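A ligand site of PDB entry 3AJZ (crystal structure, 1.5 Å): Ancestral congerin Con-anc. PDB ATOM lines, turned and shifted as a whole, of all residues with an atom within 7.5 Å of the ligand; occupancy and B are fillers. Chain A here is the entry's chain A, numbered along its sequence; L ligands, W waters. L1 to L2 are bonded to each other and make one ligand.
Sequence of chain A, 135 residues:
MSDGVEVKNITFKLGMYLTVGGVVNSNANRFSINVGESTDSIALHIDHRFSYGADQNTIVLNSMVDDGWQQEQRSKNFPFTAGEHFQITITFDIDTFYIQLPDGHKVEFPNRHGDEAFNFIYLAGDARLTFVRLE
The side-chain carboxylate (OE2) of Glu 72 lies within hydrogen-bond range of an oxygen (O3) of LIG L1 (2.6 Å). The side-chain hydroxyl (OH) of Tyr 52 is in hydrogen-bond range of an oxygen (O1) of LG2 L2 (2.8 Å). NH2 of Arg 49 sits at hydrogen-bond distance from O3 of LIG L1. An oxygen (O3) of LG2 L2 lies within hydrogen-bond range of a ring nitrogen (NE2) of His 45 (2.9 Å). O5 of LG2 L2 is in hydrogen-bond range of ND2 of Asn 62. An oxygen (O2) of LG2 L2 sits at hydrogen-bond distance from the guanidinium group (NH2) of Arg 30. O3 of LG2 L2 lies within hydrogen-bond range of OD2 of Asp 47, at 3.2 Å.
Residues that only touch the ligand: Trp 69 and Arg 74. Hydrophobic or aromatic side chains that line the ligand: His 45, Tyr 52 and Trp 69. Nine residues have an atom within 4 Å of the ligand: Arg 30, His 45, Asp 47, Arg 49, Tyr 52, Asn 62, Trp 69, Glu 72 and Arg 74. Along chain A the residues within 4 Å of the ligand span positions 30 to 74. The nearest printed residue that does not touch the ligand is Val 60 (4.5 Å).
NH1 of Arg 74 is in salt-bridge range of OE1 of Glu 72 (2.7 Å). The side-chain carboxylate of Asp 55 lies within salt-bridge range of the guanidinium group of Arg 49, at 2.9 Å. The backbone NH (N) of His 45 sits at hydrogen-bond distance from the backbone carbonyl oxygen (O) of Asn 62, at 2.8 Å. A ring nitrogen (ND1) of His 45 is in hydrogen-bond range of the side-chain amide oxygen (OD1) of Asn 34. The side-chain amide nitrogen of Asn 62 is in hydrogen-bond range of the backbone carbonyl oxygen of Gln 70 (2.8 Å). OD2 of Asp 47 is in salt-bridge range of NH2 of Arg 30 (2.8 Å). The backbone NH of Asp 47 sits at hydrogen-bond distance from the backbone carbonyl oxygen of Val 60, at 2.8 Å. NE of Arg 74 is in salt-bridge range of OD1 of Asp 55 (2.9 Å).
Water W2 lies within hydrogen-bond range of the side-chain carboxylate of Glu 72 (2.6 Å), an oxygen (O2) of LIG L1 (2.7 Å) and the guanidinium group of Arg 74 (3.4 Å). Water W4 lies within hydrogen-bond range of the side-chain carboxylate of Asp 55 (2.8 Å), the backbone NH of Ala 54 (2.9 Å) and an oxygen (O2) of LIG L1 (3.0 Å). Water W1 bridges an oxygen (O5) of LG2 L2 (3.1 Å) and the side-chain carboxylate of Glu 72 (3.2 Å).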
ATOM      1  N   ARG A  30     -17.389 -14.423  19.241  1.00  0.00           N
ATOM      2  CA  ARG A  30     -16.868 -15.453  18.337  1.00  0.00           C
ATOM      3  C   ARG A  30     -17.952 -16.489  18.092  1.00  0.00           C
ATOM      4  O   ARG A  30     -18.894 -16.657  18.887  1.00  0.00           O
ATOM      5  CB  ARG A  30     -15.648 -16.135  18.956  1.00  0.00           C
ATOM      6  CG  ARG A  30     -15.991 -16.923  20.247  1.00  0.00           C
ATOM      7  CD  ARG A  30     -14.771 -17.695  20.713  1.00  0.00           C
ATOM      8  NE  ARG A  30     -15.023 -18.400  21.972  1.00  0.00           N
ATOM      9  CZ  ARG A  30     -14.472 -19.566  22.305  1.00  0.00           C
ATOM     10  NH1 ARG A  30     -14.721 -20.084  23.493  1.00  0.00           N
ATOM     11  NH2 ARG A  30     -13.605 -20.178  21.488  1.00  0.00           N
ATOM     12  N   SER A  32     -18.029 -20.757  16.261  1.00  0.00           N
ATOM     13  CA  SER A  32     -17.273 -21.816  15.568  1.00  0.00           C
ATOM     14  C   SER A  32     -18.104 -22.814  14.772  1.00  0.00           C
ATOM     15  O   SER A  32     -19.257 -23.100  15.102  1.00  0.00           O
ATOM     16  CB  SER A  32     -16.335 -22.582  16.532  1.00  0.00           C
ATOM     17  OG  SER A  32     -17.109 -23.170  17.560  1.00  0.00           O
ATOM     18  N   ASN A  34     -17.717 -26.835  13.679  1.00  0.00           N
ATOM     19  CA  ASN A  34     -16.991 -27.973  14.279  1.00  0.00           C
ATOM     20  C   ASN A  34     -17.396 -29.211  13.543  1.00  0.00           C
ATOM     21  O   ASN A  34     -18.562 -29.590  13.649  1.00  0.00           O
ATOM     22  CB  ASN A  34     -17.372 -28.103  15.748  1.00  0.00           C
ATOM     23  CG  ASN A  34     -17.010 -26.878  16.529  1.00  0.00           C
ATOM     24  OD1 ASN A  34     -15.884 -26.779  17.017  1.00  0.00           O
ATOM     25  ND2 ASN A  34     -17.943 -25.943  16.666  1.00  0.00           N
ATOM     26  N   HIS A  45     -12.065 -27.517  13.776  1.00  0.00           N
ATOM     27  CA  HIS A  45     -12.679 -26.435  14.535  1.00  0.00           C
ATOM     28  C   HIS A  45     -12.268 -25.151  13.887  1.00  0.00           C
ATOM     29  O   HIS A  45     -11.068 -24.874  13.748  1.00  0.00           O
ATOM     30  CB  HIS A  45     -12.146 -26.505  15.970  1.00  0.00           C
ATOM     31  CG  HIS A  45     -12.468 -25.304  16.823  1.00  0.00           C
ATOM     32  ND1 HIS A  45     -13.719 -25.056  17.355  1.00  0.00           N
ATOM     33  CD2 HIS A  45     -11.643 -24.350  17.340  1.00  0.00           C
ATOM     34  CE1 HIS A  45     -13.654 -23.990  18.149  1.00  0.00           C
ATOM     35  NE2 HIS A  45     -12.411 -23.533  18.143  1.00  0.00           N
ATOM     36  N   ILE A  46     -13.244 -24.361  13.458  1.00  0.00           N
ATOM     37  CA  ILE A  46     -12.962 -23.074  12.807  1.00  0.00           C
ATOM     38  C   ILE A  46     -13.592 -22.025  13.692  1.00  0.00           C
ATOM     39  O   ILE A  46     -14.817 -21.926  13.729  1.00  0.00           O
ATOM     40  CB  ILE A  46     -13.633 -23.005  11.405  1.00  0.00           C
ATOM     41  CG1 ILE A  46     -13.359 -24.272  10.576  1.00  0.00           C
ATOM     42  CG2 ILE A  46     -13.140 -21.750  10.691  1.00  0.00           C
ATOM     43  CD1 ILE A  46     -14.293 -24.382   9.359  1.00  0.00           C
ATOM     44  N   ASP A  47     -12.767 -21.291  14.427  1.00  0.00           N
ATOM     45  CA  ASP A  47     -13.271 -20.316  15.401  1.00  0.00           C
ATOM     46  C   ASP A  47     -13.141 -18.934  14.809  1.00  0.00           C
ATOM     47  O   ASP A  47     -12.028 -18.445  14.579  1.00  0.00           O
ATOM     48  CB  ASP A  47     -12.478 -20.410  16.722  1.00  0.00           C
ATOM     49  CG  ASP A  47     -13.277 -19.958  17.930  1.00  0.00           C
ATOM     50  OD1 ASP A  47     -14.523 -19.979  17.869  1.00  0.00           O
ATOM     51  OD2 ASP A  47     -12.644 -19.568  18.927  1.00  0.00           O
ATOM     52  N   ARG A  49     -13.139 -15.402  15.412  1.00  0.00           N
ATOM     53  CA  ARG A  49     -13.013 -14.510  16.565  1.00  0.00           C
ATOM     54  C   ARG A  49     -13.085 -13.041  16.202  1.00  0.00           C
ATOM     55  O   ARG A  49     -12.106 -12.464  15.712  1.00  0.00           O
ATOM     56  CB  ARG A  49     -11.703 -14.787  17.335  1.00  0.00           C
ATOM     57  CG  ARG A  49     -11.668 -16.220  17.811  1.00  0.00           C
ATOM     58  CD  ARG A  49     -10.403 -16.501  18.609  1.00  0.00           C
ATOM     59  NE  ARG A  49     -10.472 -17.866  19.095  1.00  0.00           N
ATOM     60  CZ  ARG A  49      -9.578 -18.443  19.888  1.00  0.00           C
ATOM     61  NH1 ARG A  49      -9.760 -19.696  20.271  1.00  0.00           N
ATOM     62  NH2 ARG A  49      -8.484 -17.781  20.274  1.00  0.00           N
ATOM     63  N   TYR A  52     -11.791 -12.147  21.054  1.00  0.00           N
ATOM     64  CA  TYR A  52     -11.718 -13.182  22.054  1.00  0.00           C
ATOM     65  C   TYR A  52     -10.265 -13.370  22.418  1.00  0.00           C
ATOM     66  O   TYR A  52      -9.413 -13.516  21.542  1.00  0.00           O
ATOM     67  CB  TYR A  52     -12.320 -14.513  21.539  1.00  0.00           C
ATOM     68  CG  TYR A  52     -12.182 -15.666  22.526  1.00  0.00           C
ATOM     69  CD1 TYR A  52     -13.134 -15.875  23.524  1.00  0.00           C
ATOM     70  CD2 TYR A  52     -11.077 -16.498  22.454  1.00  0.00           C
ATOM     71  CE1 TYR A  52     -12.981 -16.916  24.449  1.00  0.00           C
ATOM     72  CE2 TYR A  52     -10.904 -17.524  23.363  1.00  0.00           C
ATOM     73  CZ  TYR A  52     -11.874 -17.733  24.339  1.00  0.00           C
ATOM     74  OH  TYR A  52     -11.666 -18.754  25.246  1.00  0.00           O
ATOM     75  N   GLY A  53      -9.962 -13.378  23.710  1.00  0.00           N
ATOM     76  CA  GLY A  53      -8.552 -13.557  24.109  1.00  0.00           C
ATOM     77  C   GLY A  53      -7.697 -12.437  23.531  1.00  0.00           C
ATOM     78  O   GLY A  53      -8.088 -11.285  23.561  1.00  0.00           O
ATOM     79  N   ALA A  54      -6.560 -12.789  22.949  1.00  0.00           N
ATOM     80  CA  ALA A  54      -5.679 -11.777  22.334  1.00  0.00           C
ATOM     81  C   ALA A  54      -5.965 -11.567  20.847  1.00  0.00           C
ATOM     82  O   ALA A  54      -5.225 -10.862  20.139  1.00  0.00           O
ATOM     83  CB  ALA A  54      -4.199 -12.110  22.588  1.00  0.00           C
ATOM     84  N   ASP A  55      -7.063 -12.169  20.379  1.00  0.00           N
ATOM     85  CA  ASP A  55      -7.401 -12.185  18.970  1.00  0.00           C
ATOM     86  C   ASP A  55      -8.511 -11.201  18.637  1.00  0.00           C
ATOM     87  O   ASP A  55      -9.567 -11.212  19.273  1.00  0.00           O
ATOM     88  CB  ASP A  55      -7.863 -13.584  18.533  1.00  0.00           C
ATOM     89  CG  ASP A  55      -6.741 -14.606  18.601  1.00  0.00           C
ATOM     90  OD1 ASP A  55      -5.702 -14.387  17.945  1.00  0.00           O
ATOM     91  OD2 ASP A  55      -6.869 -15.615  19.336  1.00  0.00           O
ATOM     92  N   VAL A  60      -9.197 -18.672  14.179  1.00  0.00           N
ATOM     93  CA  VAL A  60      -8.319 -19.638  14.832  1.00  0.00           C
ATOM     94  C   VAL A  60      -8.823 -21.020  14.485  1.00  0.00           C
ATOM     95  O   VAL A  60      -9.986 -21.339  14.724  1.00  0.00           O
ATOM     96  CB  VAL A  60      -8.313 -19.411  16.354  1.00  0.00           C
ATOM     97  CG1 VAL A  60      -7.508 -20.518  17.035  1.00  0.00           C
ATOM     98  CG2 VAL A  60      -7.740 -18.011  16.643  1.00  0.00           C
ATOM     99  N   LEU A  61      -7.947 -21.816  13.895  1.00  0.00           N
ATOM    100  CA  LEU A  61      -8.257 -23.177  13.497  1.00  0.00           C
ATOM    101  C   LEU A  61      -7.543 -24.159  14.415  1.00  0.00           C
ATOM    102  O   LEU A  61      -6.368 -23.974  14.795  1.00  0.00           O
ATOM    103  CB  LEU A  61      -7.890 -23.447  12.026  1.00  0.00           C
ATOM    104  CG  LEU A  61      -8.596 -22.478  11.074  1.00  0.00           C
ATOM    105  CD1 LEU A  61      -7.700 -21.273  10.725  1.00  0.00           C
ATOM    106  CD2 LEU A  61      -9.040 -23.233   9.839  1.00  0.00           C
ATOM    107  N   ASN A  62      -8.220 -25.226  14.762  1.00  0.00           N
ATOM    108  CA  ASN A  62      -7.615 -26.270  15.561  1.00  0.00           C
ATOM    109  C   ASN A  62      -8.399 -27.581  15.407  1.00  0.00           C
ATOM    110  O   ASN A  62      -9.375 -27.682  14.658  1.00  0.00           O
ATOM    111  CB  ASN A  62      -7.511 -25.794  17.012  1.00  0.00           C
ATOM    112  CG  ASN A  62      -6.351 -26.461  17.781  1.00  0.00           C
ATOM    113  OD1 ASN A  62      -5.679 -27.369  17.281  1.00  0.00           O
ATOM    114  ND2 ASN A  62      -6.104 -25.961  19.012  1.00  0.00           N
ATOM    115  N   SER A  63      -7.934 -28.609  16.092  1.00  0.00           N
ATOM    116  CA  SER A  63      -8.588 -29.879  16.233  1.00  0.00           C
ATOM    117  C   SER A  63      -8.551 -30.281  17.694  1.00  0.00           C
ATOM    118  O   SER A  63      -7.727 -29.753  18.465  1.00  0.00           O
ATOM    119  CB  SER A  63      -7.880 -30.946  15.387  1.00  0.00           C
ATOM    120  OG  SER A  63      -6.462 -30.923  15.663  1.00  0.00           O
ATOM    121  N   MET A  64      -9.432 -31.185  18.067  1.00  0.00           N
ATOM    122  CA  MET A  64      -9.527 -31.686  19.447  1.00  0.00           C
ATOM    123  C   MET A  64      -9.528 -33.202  19.432  1.00  0.00           C
ATOM    124  O   MET A  64     -10.328 -33.831  18.737  1.00  0.00           O
ATOM    125  CB  MET A  64     -10.811 -31.146  20.099  1.00  0.00           C
ATOM    126  CG  MET A  64     -11.269 -31.987  21.313  1.00  0.00           C
ATOM    127  SD  MET A  64     -12.803 -31.368  22.041  1.00  0.00           S
ATOM    128  CE  MET A  64     -12.232 -29.874  22.678  1.00  0.00           C
ATOM    129  N   TRP A  69      -7.357 -29.779  23.063  1.00  0.00           N
ATOM    130  CA  TRP A  69      -6.981 -28.997  21.883  1.00  0.00           C
ATOM    131  C   TRP A  69      -5.568 -29.275  21.428  1.00  0.00           C
ATOM    132  O   TRP A  69      -4.678 -29.509  22.250  1.00  0.00           O
ATOM    133  CB  TRP A  69      -7.186 -27.514  22.134  1.00  0.00           C
ATOM    134  CG  TRP A  69      -8.642 -27.164  22.318  1.00  0.00           C
ATOM    135  CD1 TRP A  69      -9.244 -26.800  23.476  1.00  0.00           C
ATOM    136  CD2 TRP A  69      -9.658 -27.167  21.314  1.00  0.00           C
ATOM    137  NE1 TRP A  69     -10.585 -26.573  23.266  1.00  0.00           N
ATOM    138  CE2 TRP A  69     -10.865 -26.793  21.944  1.00  0.00           C
ATOM    139  CE3 TRP A  69      -9.661 -27.450  19.948  1.00  0.00           C
ATOM    140  CZ2 TRP A  69     -12.086 -26.683  21.234  1.00  0.00           C
ATOM    141  CZ3 TRP A  69     -10.873 -27.333  19.240  1.00  0.00           C
ATOM    142  CH2 TRP A  69     -12.049 -26.959  19.890  1.00  0.00           C
ATOM    143  N   GLN A  70      -5.358 -29.242  20.114  1.00  0.00           N
ATOM    144  CA  GLN A  70      -4.042 -29.454  19.536  1.00  0.00           C
ATOM    145  C   GLN A  70      -3.415 -28.103  19.175  1.00  0.00           C
ATOM    146  O   GLN A  70      -3.701 -27.103  19.858  1.00  0.00           O
ATOM    147  CB  GLN A  70      -4.141 -30.441  18.354  1.00  0.00           C
ATOM    148  CG  GLN A  70      -4.737 -31.810  18.734  1.00  0.00           C
ATOM    149  CD  GLN A  70      -4.588 -32.871  17.589  1.00  0.00           C
ATOM    150  OE1 GLN A  70      -5.382 -32.919  16.632  1.00  0.00           O
ATOM    151  NE2 GLN A  70      -3.586 -33.742  17.723  1.00  0.00           N
ATOM    152  N   GLN A  71      -2.548 -28.037  18.170  1.00  0.00           N
ATOM    153  CA  GLN A  71      -1.850 -26.788  17.865  1.00  0.00           C
ATOM    154  C   GLN A  71      -2.701 -25.852  16.997  1.00  0.00           C
ATOM    155  O   GLN A  71      -3.206 -26.221  15.912  1.00  0.00           O
ATOM    156  CB  GLN A  71      -0.497 -27.059  17.184  1.00  0.00           C
ATOM    157  CG  GLN A  71       0.324 -25.789  16.924  1.00  0.00           C
ATOM    158  CD  GLN A  71       1.818 -26.068  16.696  1.00  0.00           C
ATOM    159  OE1 GLN A  71       2.233 -27.196  16.379  1.00  0.00           O
ATOM    160  NE2 GLN A  71       2.629 -25.023  16.854  1.00  0.00           N
ATOM    161  N   GLU A  72      -2.838 -24.621  17.449  1.00  0.00           N
ATOM    162  CA  GLU A  72      -3.577 -23.599  16.715  1.00  0.00           C
ATOM    163  C   GLU A  72      -2.892 -23.130  15.481  1.00  0.00           C
ATOM    164  O   GLU A  72      -1.635 -23.077  15.393  1.00  0.00           O
ATOM    165  CB  GLU A  72      -3.834 -22.386  17.615  1.00  0.00           C
ATOM    166  CG  GLU A  72      -4.754 -22.711  18.737  1.00  0.00           C
ATOM    167  CD  GLU A  72      -4.953 -21.569  19.738  1.00  0.00           C
ATOM    168  OE1 GLU A  72      -4.253 -20.534  19.667  1.00  0.00           O
ATOM    169  OE2 GLU A  72      -5.830 -21.705  20.615  1.00  0.00           O
ATOM    170  N   GLN A  73      -3.722 -22.814  14.487  1.00  0.00           N
ATOM    171  CA  GLN A  73      -3.290 -22.097  13.316  1.00  0.00           C
ATOM    172  C   GLN A  73      -4.188 -20.894  13.177  1.00  0.00           C
ATOM    173  O   GLN A  73      -5.325 -20.889  13.668  1.00  0.00           O
ATOM    174  CB  GLN A  73      -3.380 -22.984  12.078  1.00  0.00           C
ATOM    175  CG  GLN A  73      -2.440 -24.207  12.174  1.00  0.00           C
ATOM    176  CD  GLN A  73      -2.283 -25.010  10.893  1.00  0.00           C
ATOM    177  OE1 GLN A  73      -2.885 -24.723   9.812  1.00  0.00           O
ATOM    178  NE2 GLN A  73      -1.435 -26.045  11.004  1.00  0.00           N
ATOM    179  N   ARG A  74      -3.680 -19.843  12.557  1.00  0.00           N
ATOM    180  CA  ARG A  74      -4.432 -18.596  12.461  1.00  0.00           C
ATOM    181  C   ARG A  74      -4.495 -18.110  11.046  1.00  0.00           C
ATOM    182  O   ARG A  74      -3.559 -18.323  10.259  1.00  0.00           O
ATOM    183  CB  ARG A  74      -3.854 -17.510  13.362  1.00  0.00           C
ATOM    184  CG  ARG A  74      -4.272 -17.678  14.835  1.00  0.00           C
ATOM    185  CD  ARG A  74      -3.584 -16.707  15.814  1.00  0.00           C
ATOM    186  NE  ARG A  74      -4.241 -16.739  17.121  1.00  0.00           N
ATOM    187  CZ  ARG A  74      -4.195 -17.771  17.960  1.00  0.00           C
ATOM    188  NH1 ARG A  74      -3.480 -18.847  17.668  1.00  0.00           N
ATOM    189  NH2 ARG A  74      -4.893 -17.719  19.088  1.00  0.00           N
HETATM  190  C1  LIG L   1      -5.324 -19.097  23.521  1.00  0.00           C
HETATM  191  C2  LIG L   1      -6.777 -19.295  23.077  1.00  0.00           C
HETATM  192  C3  LIG L   1      -7.449 -20.452  23.809  1.00  0.00           C
HETATM  193  C4  LIG L   1      -7.272 -20.150  25.306  1.00  0.00           C
HETATM  194  C5  LIG L   1      -7.886 -21.193  26.234  1.00  0.00           C
HETATM  195  C6  LIG L   1      -5.314 -18.905  25.032  1.00  0.00           C
HETATM  196  O1  LIG L   1      -3.987 -18.876  25.493  1.00  0.00           O
HETATM  197  O2  LIG L   1      -4.777 -17.960  22.903  1.00  0.00           O
HETATM  198  O3  LIG L   1      -6.833 -19.526  21.681  1.00  0.00           O
HETATM  199  O4  LIG L   1      -8.832 -20.447  23.521  1.00  0.00           O
HETATM  200  O5  LIG L   1      -5.887 -20.068  25.589  1.00  0.00           O
HETATM  201  O6  LIG L   1      -7.339 -22.451  25.921  1.00  0.00           O
HETATM  202  C1  LG2 L   2      -9.374 -21.725  23.138  1.00  0.00           C
HETATM  203  C2  LG2 L   2     -10.905 -21.653  23.275  1.00  0.00           C
HETATM  204  C3  LG2 L   2     -11.571 -22.924  22.746  1.00  0.00           C
HETATM  205  C4  LG2 L   2     -11.060 -23.183  21.321  1.00  0.00           C
HETATM  206  C5  LG2 L   2      -9.530 -23.279  21.397  1.00  0.00           C
HETATM  207  C6  LG2 L   2      -8.923 -23.555  20.031  1.00  0.00           C
HETATM  208  O1  LG2 L   2     -11.292 -21.429  24.635  1.00  0.00           O
HETATM  209  O2  LG2 L   2     -12.962 -22.763  22.763  1.00  0.00           O
HETATM  210  O3  LG2 L   2     -11.524 -22.135  20.468  1.00  0.00           O
HETATM  211  O4  LG2 L   2      -8.946 -22.045  21.829  1.00  0.00           O
HETATM  212  O5  LG2 L   2      -7.526 -23.749  20.147  1.00  0.00           O
HETATM  213  O   HOH W   1      -5.758 -24.081  22.707  1.00  0.00           O
HETATM  214  O   HOH W   2      -2.838 -19.166  21.381  1.00  0.00           O
HETATM  215  O   HOH W   3     -15.254 -23.468  21.194  1.00  0.00           O
HETATM  216  O   HOH W   4      -6.128 -15.484  22.006  1.00  0.00           O
